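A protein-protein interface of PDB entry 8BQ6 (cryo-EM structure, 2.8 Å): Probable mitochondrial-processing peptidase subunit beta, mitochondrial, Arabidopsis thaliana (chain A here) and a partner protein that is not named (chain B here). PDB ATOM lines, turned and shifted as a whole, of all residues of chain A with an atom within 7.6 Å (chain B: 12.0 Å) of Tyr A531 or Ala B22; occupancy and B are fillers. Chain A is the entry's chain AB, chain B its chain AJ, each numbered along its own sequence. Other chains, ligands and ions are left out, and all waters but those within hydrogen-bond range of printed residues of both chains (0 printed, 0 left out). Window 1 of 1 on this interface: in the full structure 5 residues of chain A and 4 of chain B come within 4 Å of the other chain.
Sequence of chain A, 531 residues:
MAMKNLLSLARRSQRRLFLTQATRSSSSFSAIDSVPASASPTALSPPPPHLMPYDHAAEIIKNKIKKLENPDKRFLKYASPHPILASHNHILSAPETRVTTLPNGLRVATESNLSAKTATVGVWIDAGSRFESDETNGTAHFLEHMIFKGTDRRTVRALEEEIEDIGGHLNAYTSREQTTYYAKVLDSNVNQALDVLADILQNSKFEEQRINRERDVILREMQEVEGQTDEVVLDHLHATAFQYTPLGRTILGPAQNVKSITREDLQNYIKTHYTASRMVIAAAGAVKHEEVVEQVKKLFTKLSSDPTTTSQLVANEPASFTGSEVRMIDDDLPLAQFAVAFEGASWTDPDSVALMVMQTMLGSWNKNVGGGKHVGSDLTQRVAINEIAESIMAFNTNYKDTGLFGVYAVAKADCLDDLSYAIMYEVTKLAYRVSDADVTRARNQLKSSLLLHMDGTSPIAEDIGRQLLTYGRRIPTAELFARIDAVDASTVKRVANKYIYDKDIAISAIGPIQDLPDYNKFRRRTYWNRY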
ATOM      1  N   TYR A 425     -24.183  16.861   3.341  1.00  0.00           N
ATOM      2  CA  TYR A 425     -23.448  15.696   2.862  1.00  0.00           C
ATOM      3  C   TYR A 425     -22.843  14.910   4.017  1.00  0.00           C
ATOM      4  O   TYR A 425     -22.895  13.675   4.039  1.00  0.00           O
ATOM      5  CB  TYR A 425     -22.359  16.125   1.879  1.00  0.00           C
ATOM      6  CG  TYR A 425     -21.639  14.957   1.251  1.00  0.00           C
ATOM      7  CD1 TYR A 425     -22.094  14.391   0.072  1.00  0.00           C
ATOM      8  CD2 TYR A 425     -20.512  14.408   1.848  1.00  0.00           C
ATOM      9  CE1 TYR A 425     -21.443  13.322  -0.502  1.00  0.00           C
ATOM     10  CE2 TYR A 425     -19.859  13.336   1.285  1.00  0.00           C
ATOM     11  CZ  TYR A 425     -20.327  12.799   0.109  1.00  0.00           C
ATOM     12  OH  TYR A 425     -19.677  11.731  -0.459  1.00  0.00           O
ATOM     13  N   ALA A 431     -25.355   7.873   7.800  1.00  0.00           N
ATOM     14  CA  ALA A 431     -26.232   6.727   7.609  1.00  0.00           C
ATOM     15  C   ALA A 431     -25.669   5.701   6.638  1.00  0.00           C
ATOM     16  O   ALA A 431     -26.253   4.621   6.500  1.00  0.00           O
ATOM     17  CB  ALA A 431     -27.606   7.188   7.117  1.00  0.00           C
ATOM     18  N   TYR A 432     -24.568   6.013   5.954  1.00  0.00           N
ATOM     19  CA  TYR A 432     -24.014   5.129   4.937  1.00  0.00           C
ATOM     20  C   TYR A 432     -22.601   4.662   5.245  1.00  0.00           C
ATOM     21  O   TYR A 432     -22.356   3.454   5.305  1.00  0.00           O
ATOM     22  CB  TYR A 432     -24.036   5.834   3.576  1.00  0.00           C
ATOM     23  CG  TYR A 432     -25.415   6.186   3.079  1.00  0.00           C
ATOM     24  CD1 TYR A 432     -26.228   5.229   2.491  1.00  0.00           C
ATOM     25  CD2 TYR A 432     -25.904   7.478   3.198  1.00  0.00           C
ATOM     26  CE1 TYR A 432     -27.487   5.554   2.031  1.00  0.00           C
ATOM     27  CE2 TYR A 432     -27.158   7.810   2.744  1.00  0.00           C
ATOM     28  CZ  TYR A 432     -27.946   6.847   2.162  1.00  0.00           C
ATOM     29  OH  TYR A 432     -29.197   7.183   1.709  1.00  0.00           O
ATOM     30  N   ARG A 433     -21.659   5.581   5.455  1.00  0.00           N
ATOM     31  CA  ARG A 433     -20.246   5.234   5.597  1.00  0.00           C
ATOM     32  C   ARG A 433     -19.691   5.817   6.885  1.00  0.00           C
ATOM     33  O   ARG A 433     -19.465   7.028   6.976  1.00  0.00           O
ATOM     34  CB  ARG A 433     -19.426   5.725   4.408  1.00  0.00           C
ATOM     35  CG  ARG A 433     -19.151   4.670   3.365  1.00  0.00           C
ATOM     36  CD  ARG A 433     -18.364   5.247   2.202  1.00  0.00           C
ATOM     37  NE  ARG A 433     -19.225   5.809   1.169  1.00  0.00           N
ATOM     38  CZ  ARG A 433     -19.324   7.104   0.897  1.00  0.00           C
ATOM     39  NH1 ARG A 433     -18.634   8.007   1.573  1.00  0.00           N
ATOM     40  NH2 ARG A 433     -20.129   7.501  -0.084  1.00  0.00           N
ATOM     41  N   TYR A 501     -31.840   9.865   8.276  1.00  0.00           N
ATOM     42  CA  TYR A 501     -32.123   9.447   6.912  1.00  0.00           C
ATOM     43  C   TYR A 501     -33.579   9.711   6.537  1.00  0.00           C
ATOM     44  O   TYR A 501     -34.500   9.196   7.176  1.00  0.00           O
ATOM     45  CB  TYR A 501     -31.789   7.967   6.748  1.00  0.00           C
ATOM     46  CG  TYR A 501     -32.240   7.410   5.433  1.00  0.00           C
ATOM     47  CD1 TYR A 501     -31.484   7.587   4.288  1.00  0.00           C
ATOM     48  CD2 TYR A 501     -33.434   6.721   5.331  1.00  0.00           C
ATOM     49  CE1 TYR A 501     -31.905   7.086   3.083  1.00  0.00           C
ATOM     50  CE2 TYR A 501     -33.862   6.222   4.135  1.00  0.00           C
ATOM     51  CZ  TYR A 501     -33.097   6.406   3.011  1.00  0.00           C
ATOM     52  OH  TYR A 501     -33.531   5.899   1.813  1.00  0.00           O
ATOM     53  N   TYR A 527     -31.060  12.089   1.942  1.00  0.00           N
ATOM     54  CA  TYR A 527     -30.848  10.726   1.483  1.00  0.00           C
ATOM     55  C   TYR A 527     -29.995  10.757   0.225  1.00  0.00           C
ATOM     56  O   TYR A 527     -29.895  11.777  -0.462  1.00  0.00           O
ATOM     57  CB  TYR A 527     -32.175   9.997   1.228  1.00  0.00           C
ATOM     58  CG  TYR A 527     -33.142  10.764   0.362  1.00  0.00           C
ATOM     59  CD1 TYR A 527     -34.069  11.626   0.927  1.00  0.00           C
ATOM     60  CD2 TYR A 527     -33.130  10.627  -1.017  1.00  0.00           C
ATOM     61  CE1 TYR A 527     -34.951  12.331   0.149  1.00  0.00           C
ATOM     62  CE2 TYR A 527     -34.011  11.328  -1.806  1.00  0.00           C
ATOM     63  CZ  TYR A 527     -34.921  12.179  -1.217  1.00  0.00           C
ATOM     64  OH  TYR A 527     -35.805  12.885  -1.992  1.00  0.00           O
ATOM     65  N   TRP A 528     -29.364   9.626  -0.065  1.00  0.00           N
ATOM     66  CA  TRP A 528     -28.545   9.461  -1.258  1.00  0.00           C
ATOM     67  C   TRP A 528     -29.243   8.475  -2.180  1.00  0.00           C
ATOM     68  O   TRP A 528     -29.555   7.351  -1.772  1.00  0.00           O
ATOM     69  CB  TRP A 528     -27.140   8.974  -0.902  1.00  0.00           C
ATOM     70  CG  TRP A 528     -26.277  10.015  -0.257  1.00  0.00           C
ATOM     71  CD1 TRP A 528     -26.540  11.347  -0.146  1.00  0.00           C
ATOM     72  CD2 TRP A 528     -25.007   9.804   0.367  1.00  0.00           C
ATOM     73  NE1 TRP A 528     -25.513  11.979   0.507  1.00  0.00           N
ATOM     74  CE2 TRP A 528     -24.559  11.052   0.833  1.00  0.00           C
ATOM     75  CE3 TRP A 528     -24.207   8.679   0.577  1.00  0.00           C
ATOM     76  CZ2 TRP A 528     -23.350  11.208   1.495  1.00  0.00           C
ATOM     77  CZ3 TRP A 528     -23.009   8.836   1.235  1.00  0.00           C
ATOM     78  CH2 TRP A 528     -22.589  10.090   1.685  1.00  0.00           C
ATOM     79  N   ASN A 529     -29.490   8.896  -3.418  1.00  0.00           N
ATOM     80  CA  ASN A 529     -30.197   8.052  -4.368  1.00  0.00           C
ATOM     81  C   ASN A 529     -29.285   7.060  -5.080  1.00  0.00           C
ATOM     82  O   ASN A 529     -29.785   6.219  -5.832  1.00  0.00           O
ATOM     83  CB  ASN A 529     -30.925   8.923  -5.392  1.00  0.00           C
ATOM     84  CG  ASN A 529     -32.386   9.123  -5.046  1.00  0.00           C
ATOM     85  OD1 ASN A 529     -32.943   8.400  -4.224  1.00  0.00           O
ATOM     86  ND2 ASN A 529     -33.010  10.114  -5.666  1.00  0.00           N
ATOM     87  N   ARG A 530     -27.975   7.121  -4.858  1.00  0.00           N
ATOM     88  CA  ARG A 530     -27.072   6.142  -5.447  1.00  0.00           C
ATOM     89  C   ARG A 530     -26.970   4.868  -4.623  1.00  0.00           C
ATOM     90  O   ARG A 530     -26.153   4.001  -4.950  1.00  0.00           O
ATOM     91  CB  ARG A 530     -25.678   6.742  -5.636  1.00  0.00           C
ATOM     92  CG  ARG A 530     -24.952   7.079  -4.348  1.00  0.00           C
ATOM     93  CD  ARG A 530     -23.825   8.050  -4.637  1.00  0.00           C
ATOM     94  NE  ARG A 530     -23.114   8.465  -3.435  1.00  0.00           N
ATOM     95  CZ  ARG A 530     -23.151   9.692  -2.938  1.00  0.00           C
ATOM     96  NH1 ARG A 530     -23.888  10.640  -3.493  1.00  0.00           N
ATOM     97  NH2 ARG A 530     -22.430   9.978  -1.859  1.00  0.00           N
ATOM     98  N   TYR A 531     -27.767   4.741  -3.569  1.00  0.00           N
ATOM     99  CA  TYR A 531     -27.735   3.573  -2.701  1.00  0.00           C
ATOM    100  C   TYR A 531     -29.112   2.926  -2.604  1.00  0.00           C
ATOM    101  O   TYR A 531     -29.816   2.784  -3.602  1.00  0.00           O
ATOM    102  CB  TYR A 531     -27.242   3.959  -1.309  1.00  0.00           C
ATOM    103  CG  TYR A 531     -25.746   4.127  -1.201  1.00  0.00           C
ATOM    104  CD1 TYR A 531     -24.888   3.072  -1.474  1.00  0.00           C
ATOM    105  CD2 TYR A 531     -25.192   5.340  -0.823  1.00  0.00           C
ATOM    106  CE1 TYR A 531     -23.519   3.224  -1.372  1.00  0.00           C
ATOM    107  CE2 TYR A 531     -23.827   5.500  -0.717  1.00  0.00           C
ATOM    108  CZ  TYR A 531     -22.996   4.441  -0.993  1.00  0.00           C
ATOM    109  OH  TYR A 531     -21.636   4.604  -0.890  1.00  0.00           O
ATOM    110  N   THR B  17     -19.325  -1.795   4.270  1.00  0.00           N
ATOM    111  CA  THR B  17     -19.604  -3.045   3.574  1.00  0.00           C
ATOM    112  C   THR B  17     -20.895  -2.926   2.778  1.00  0.00           C
ATOM    113  O   THR B  17     -21.544  -3.925   2.472  1.00  0.00           O
ATOM    114  CB  THR B  17     -19.720  -4.227   4.551  1.00  0.00           C
ATOM    115  OG1 THR B  17     -20.827  -4.010   5.433  1.00  0.00           O
ATOM    116  CG2 THR B  17     -18.446  -4.369   5.369  1.00  0.00           C
ATOM    117  N   ILE B  18     -21.263  -1.690   2.450  1.00  0.00           N
ATOM    118  CA  ILE B  18     -22.509  -1.421   1.742  1.00  0.00           C
ATOM    119  C   ILE B  18     -22.327  -1.367   0.229  1.00  0.00           C
ATOM    120  O   ILE B  18     -23.254  -1.744  -0.506  1.00  0.00           O
ATOM    121  CB  ILE B  18     -23.146  -0.118   2.276  1.00  0.00           C
ATOM    122  CG1 ILE B  18     -23.743  -0.371   3.662  1.00  0.00           C
ATOM    123  CG2 ILE B  18     -24.200   0.441   1.323  1.00  0.00           C
ATOM    124  CD1 ILE B  18     -23.888   0.863   4.511  1.00  0.00           C
ATOM    125  N   ASP B  19     -21.154  -0.953  -0.256  1.00  0.00           N
ATOM    126  CA  ASP B  19     -20.930  -0.853  -1.695  1.00  0.00           C
ATOM    127  C   ASP B  19     -21.223  -2.181  -2.391  1.00  0.00           C
ATOM    128  O   ASP B  19     -21.743  -2.200  -3.513  1.00  0.00           O
ATOM    129  CB  ASP B  19     -19.492  -0.387  -1.953  1.00  0.00           C
ATOM    130  CG  ASP B  19     -19.260   1.069  -1.580  1.00  0.00           C
ATOM    131  OD1 ASP B  19     -20.248   1.810  -1.391  1.00  0.00           O
ATOM    132  OD2 ASP B  19     -18.085   1.475  -1.466  1.00  0.00           O
ATOM    133  N   ILE B  20     -20.914  -3.304  -1.736  1.00  0.00           N
ATOM    134  CA  ILE B  20     -21.268  -4.601  -2.304  1.00  0.00           C
ATOM    135  C   ILE B  20     -22.780  -4.801  -2.287  1.00  0.00           C
ATOM    136  O   ILE B  20     -23.336  -5.485  -3.153  1.00  0.00           O
ATOM    137  CB  ILE B  20     -20.530  -5.741  -1.572  1.00  0.00           C
ATOM    138  CG1 ILE B  20     -21.323  -6.211  -0.351  1.00  0.00           C
ATOM    139  CG2 ILE B  20     -19.120  -5.309  -1.186  1.00  0.00           C
ATOM    140  CD1 ILE B  20     -20.680  -7.336   0.398  1.00  0.00           C
ATOM    141  N   GLN B  21     -23.473  -4.217  -1.305  1.00  0.00           N
ATOM    142  CA  GLN B  21     -24.927  -4.334  -1.282  1.00  0.00           C
ATOM    143  C   GLN B  21     -25.569  -3.404  -2.299  1.00  0.00           C
ATOM    144  O   GLN B  21     -26.599  -3.738  -2.895  1.00  0.00           O
ATOM    145  CB  GLN B  21     -25.467  -4.041   0.113  1.00  0.00           C
ATOM    146  CG  GLN B  21     -24.677  -4.675   1.222  1.00  0.00           C
ATOM    147  CD  GLN B  21     -25.463  -4.744   2.507  1.00  0.00           C
ATOM    148  OE1 GLN B  21     -26.121  -3.781   2.899  1.00  0.00           O
ATOM    149  NE2 GLN B  21     -25.403  -5.890   3.174  1.00  0.00           N
ATOM    150  N   ALA B  22     -24.987  -2.220  -2.497  1.00  0.00           N
ATOM    151  CA  ALA B  22     -25.503  -1.320  -3.521  1.00  0.00           C
ATOM    152  C   ALA B  22     -25.251  -1.884  -4.911  1.00  0.00           C
ATOM    153  O   ALA B  22     -26.071  -1.709  -5.819  1.00  0.00           O
ATOM    154  CB  ALA B  22     -24.874   0.064  -3.374  1.00  0.00           C
ATOM    155  N   ALA B  23     -24.116  -2.561  -5.098  1.00  0.00           N
ATOM    156  CA  ALA B  23     -23.856  -3.233  -6.367  1.00  0.00           C
ATOM    157  C   ALA B  23     -24.855  -4.357  -6.609  1.00  0.00           C
ATOM    158  O   ALA B  23     -25.387  -4.496  -7.716  1.00  0.00           O
ATOM    159  CB  ALA B  23     -22.426  -3.770  -6.395  1.00  0.00           C
ATOM    160  N   ALA B  24     -25.127  -5.166  -5.581  1.00  0.00           N
ATOM    161  CA  ALA B  24     -26.067  -6.270  -5.741  1.00  0.00           C
ATOM    162  C   ALA B  24     -27.486  -5.763  -5.961  1.00  0.00           C
ATOM    163  O   ALA B  24     -28.275  -6.394  -6.675  1.00  0.00           O
ATOM    164  CB  ALA B  24     -26.009  -7.194  -4.523  1.00  0.00           C
ATOM    165  N   GLY B  25     -27.833  -4.630  -5.352  1.00  0.00           N
ATOM    166  CA  GLY B  25     -29.179  -4.103  -5.512  1.00  0.00           C
ATOM    167  C   GLY B  25     -29.367  -3.388  -6.836  1.00  0.00           C
ATOM    168  O   GLY B  25     -30.480  -3.302  -7.359  1.00  0.00           O
ATOM    169  N   TRP B  26     -28.274  -2.861  -7.395  1.00  0.00           N
ATOM    170  CA  TRP B  26     -28.359  -2.215  -8.699  1.00  0.00           C
ATOM    171  C   TRP B  26     -28.230  -3.224  -9.833  1.00  0.00           C
ATOM    172  O   TRP B  26     -28.673  -2.955 -10.955  1.00  0.00           O
ATOM    173  CB  TRP B  26     -27.289  -1.133  -8.826  1.00  0.00           C
ATOM    174  CG  TRP B  26     -27.654   0.168  -8.174  1.00  0.00           C
ATOM    175  CD1 TRP B  26     -26.943   0.828  -7.215  1.00  0.00           C
ATOM    176  CD2 TRP B  26     -28.814   0.969  -8.433  1.00  0.00           C
ATOM    177  NE1 TRP B  26     -27.587   1.987  -6.861  1.00  0.00           N
ATOM    178  CE2 TRP B  26     -28.738   2.097  -7.595  1.00  0.00           C
ATOM    179  CE3 TRP B  26     -29.910   0.841  -9.292  1.00  0.00           C
ATOM    180  CZ2 TRP B  26     -29.715   3.089  -7.587  1.00  0.00           C
ATOM    181  CZ3 TRP B  26     -30.876   1.826  -9.285  1.00  0.00           C
ATOM    182  CH2 TRP B  26     -30.774   2.935  -8.439  1.00  0.00           C
ATOM    183  N   GLY B  27     -27.601  -4.371  -9.572  1.00  0.00           N
ATOM    184  CA  GLY B  27     -27.626  -5.451 -10.543  1.00  0.00           C
ATOM    185  C   GLY B  27     -29.005  -6.068 -10.674  1.00  0.00           C
ATOM    186  O   GLY B  27     -29.434  -6.428 -11.774  1.00  0.00           O
ATOM    187  N   ILE B  28     -29.711  -6.211  -9.551  1.00  0.00           N
ATOM    188  CA  ILE B  28     -31.089  -6.691  -9.587  1.00  0.00           C
ATOM    189  C   ILE B  28     -31.969  -5.705 -10.341  1.00  0.00           C
ATOM    190  O   ILE B  28     -32.857  -6.099 -11.109  1.00  0.00           O
ATOM    191  CB  ILE B  28     -31.598  -6.939  -8.153  1.00  0.00           C
ATOM    192  CG1 ILE B  28     -30.854  -8.127  -7.534  1.00  0.00           C
ATOM    193  CG2 ILE B  28     -33.105  -7.163  -8.142  1.00  0.00           C
ATOM    194  CD1 ILE B  28     -31.560  -8.769  -6.361  1.00  0.00           C
ATOM    195  N   ALA B  29     -31.737  -4.407 -10.138  1.00  0.00           N
ATOM    196  CA  ALA B  29     -32.470  -3.396 -10.893  1.00  0.00           C
ATOM    197  C   ALA B  29     -32.132  -3.466 -12.377  1.00  0.00           C
ATOM    198  O   ALA B  29     -33.012  -3.305 -13.230  1.00  0.00           O
ATOM    199  CB  ALA B  29     -32.170  -2.006 -10.334  1.00  0.00           C
ATOM    200  N   ALA B  30     -30.857  -3.697 -12.703  1.00  0.00           N
ATOM    201  CA  ALA B  30     -30.460  -3.849 -14.098  1.00  0.00           C
ATOM    202  C   ALA B  30     -31.066  -5.101 -14.717  1.00  0.00           C
ATOM    203  O   ALA B  30     -31.493  -5.082 -15.877  1.00  0.00           O
ATOM    204  CB  ALA B  30     -28.936  -3.883 -14.211  1.00  0.00           C
ATOM    205  N   ALA B  31     -31.096  -6.205 -13.966  1.00  0.00           N
ATOM    206  CA  ALA B  31     -31.644  -7.449 -14.499  1.00  0.00           C
ATOM    207  C   ALA B  31     -33.151  -7.348 -14.698  1.00  0.00           C
ATOM    208  O   ALA B  31     -33.688  -7.823 -15.704  1.00  0.00           O
ATOM    209  CB  ALA B  31     -31.294  -8.615 -13.575  1.00  0.00           C
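Of the printed residues of chain B, Tyr A531 touches Ile B18, Asp B19, Ala B22 and Trp B26. Of the printed residues of chain A, Ala B22 touches Tyr A531 (3.6 Å). Printed residues of chain B within 4 Å of Tyr A432: Ile B18. Trp A528 touches none of the printed residues of chain B. Asn A529 touches one residue of chain B. Of the printed residues of chain A, Asp B19 touches Tyr A531 (3.2 Å). Printed residues of chain A within 4 Å of Trp B26: Asn A529 (3.6 Å), Arg A530 (3.1 Å) and Tyr A531 (3.998 Å). Of the printed residues of chain A, Ile B18 touches Tyr A432 (3.1 Å) and Tyr A531 (3.9 Å). Tyr A425 touches none of the printed residues of chain B. Tyr A527 touches none of the printed residues of chain B. The nearest printed residue of chain A that does not touch Asp B19 is Arg A433 (4.9 Å).
The side-chain hydroxyl (OH) of Tyr A432 lies within hydrogen-bond range of the backbone NH (N) of Trp A528, 3.0 Å away. The guanidinium group of Arg A433 lies within hydrogen-bond range of the side-chain hydroxyl of Tyr A531 (3.4 Å).
O of Arg A530 sits at hydrogen-bond distance from NE1 of Trp B26. OH of Tyr A531 sits at hydrogen-bond distance from OD1 of Asp B19.
Tyr A432 touches Ile B18. O of Asn A529 touches CZ2 of Trp B26 (3.6 Å). CD1 of Tyr A531 touches CG2 of Ile B18, 3.9 Å away. Tyr A531 touches Ala B22. Tyr A531 touches Trp B26.
Of the 15 printed residues of chain B, 4 touch a printed residue of chain A. Printed residues of chain B that touch a printed residue of chain A: Ile B18, Asp B19, Ala B22 and Trp B26. Hydrophobic or aromatic side chains of chain B within 4 Å of the printed part of chain A: Ile B18, Ala B22 and Trp B26. Printed residues of chain A that touch a printed residue of chain B: Tyr A432, Asn A529, Arg A530 and Tyr A531. Among the printed residues, 7 pairs touch across the chains.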
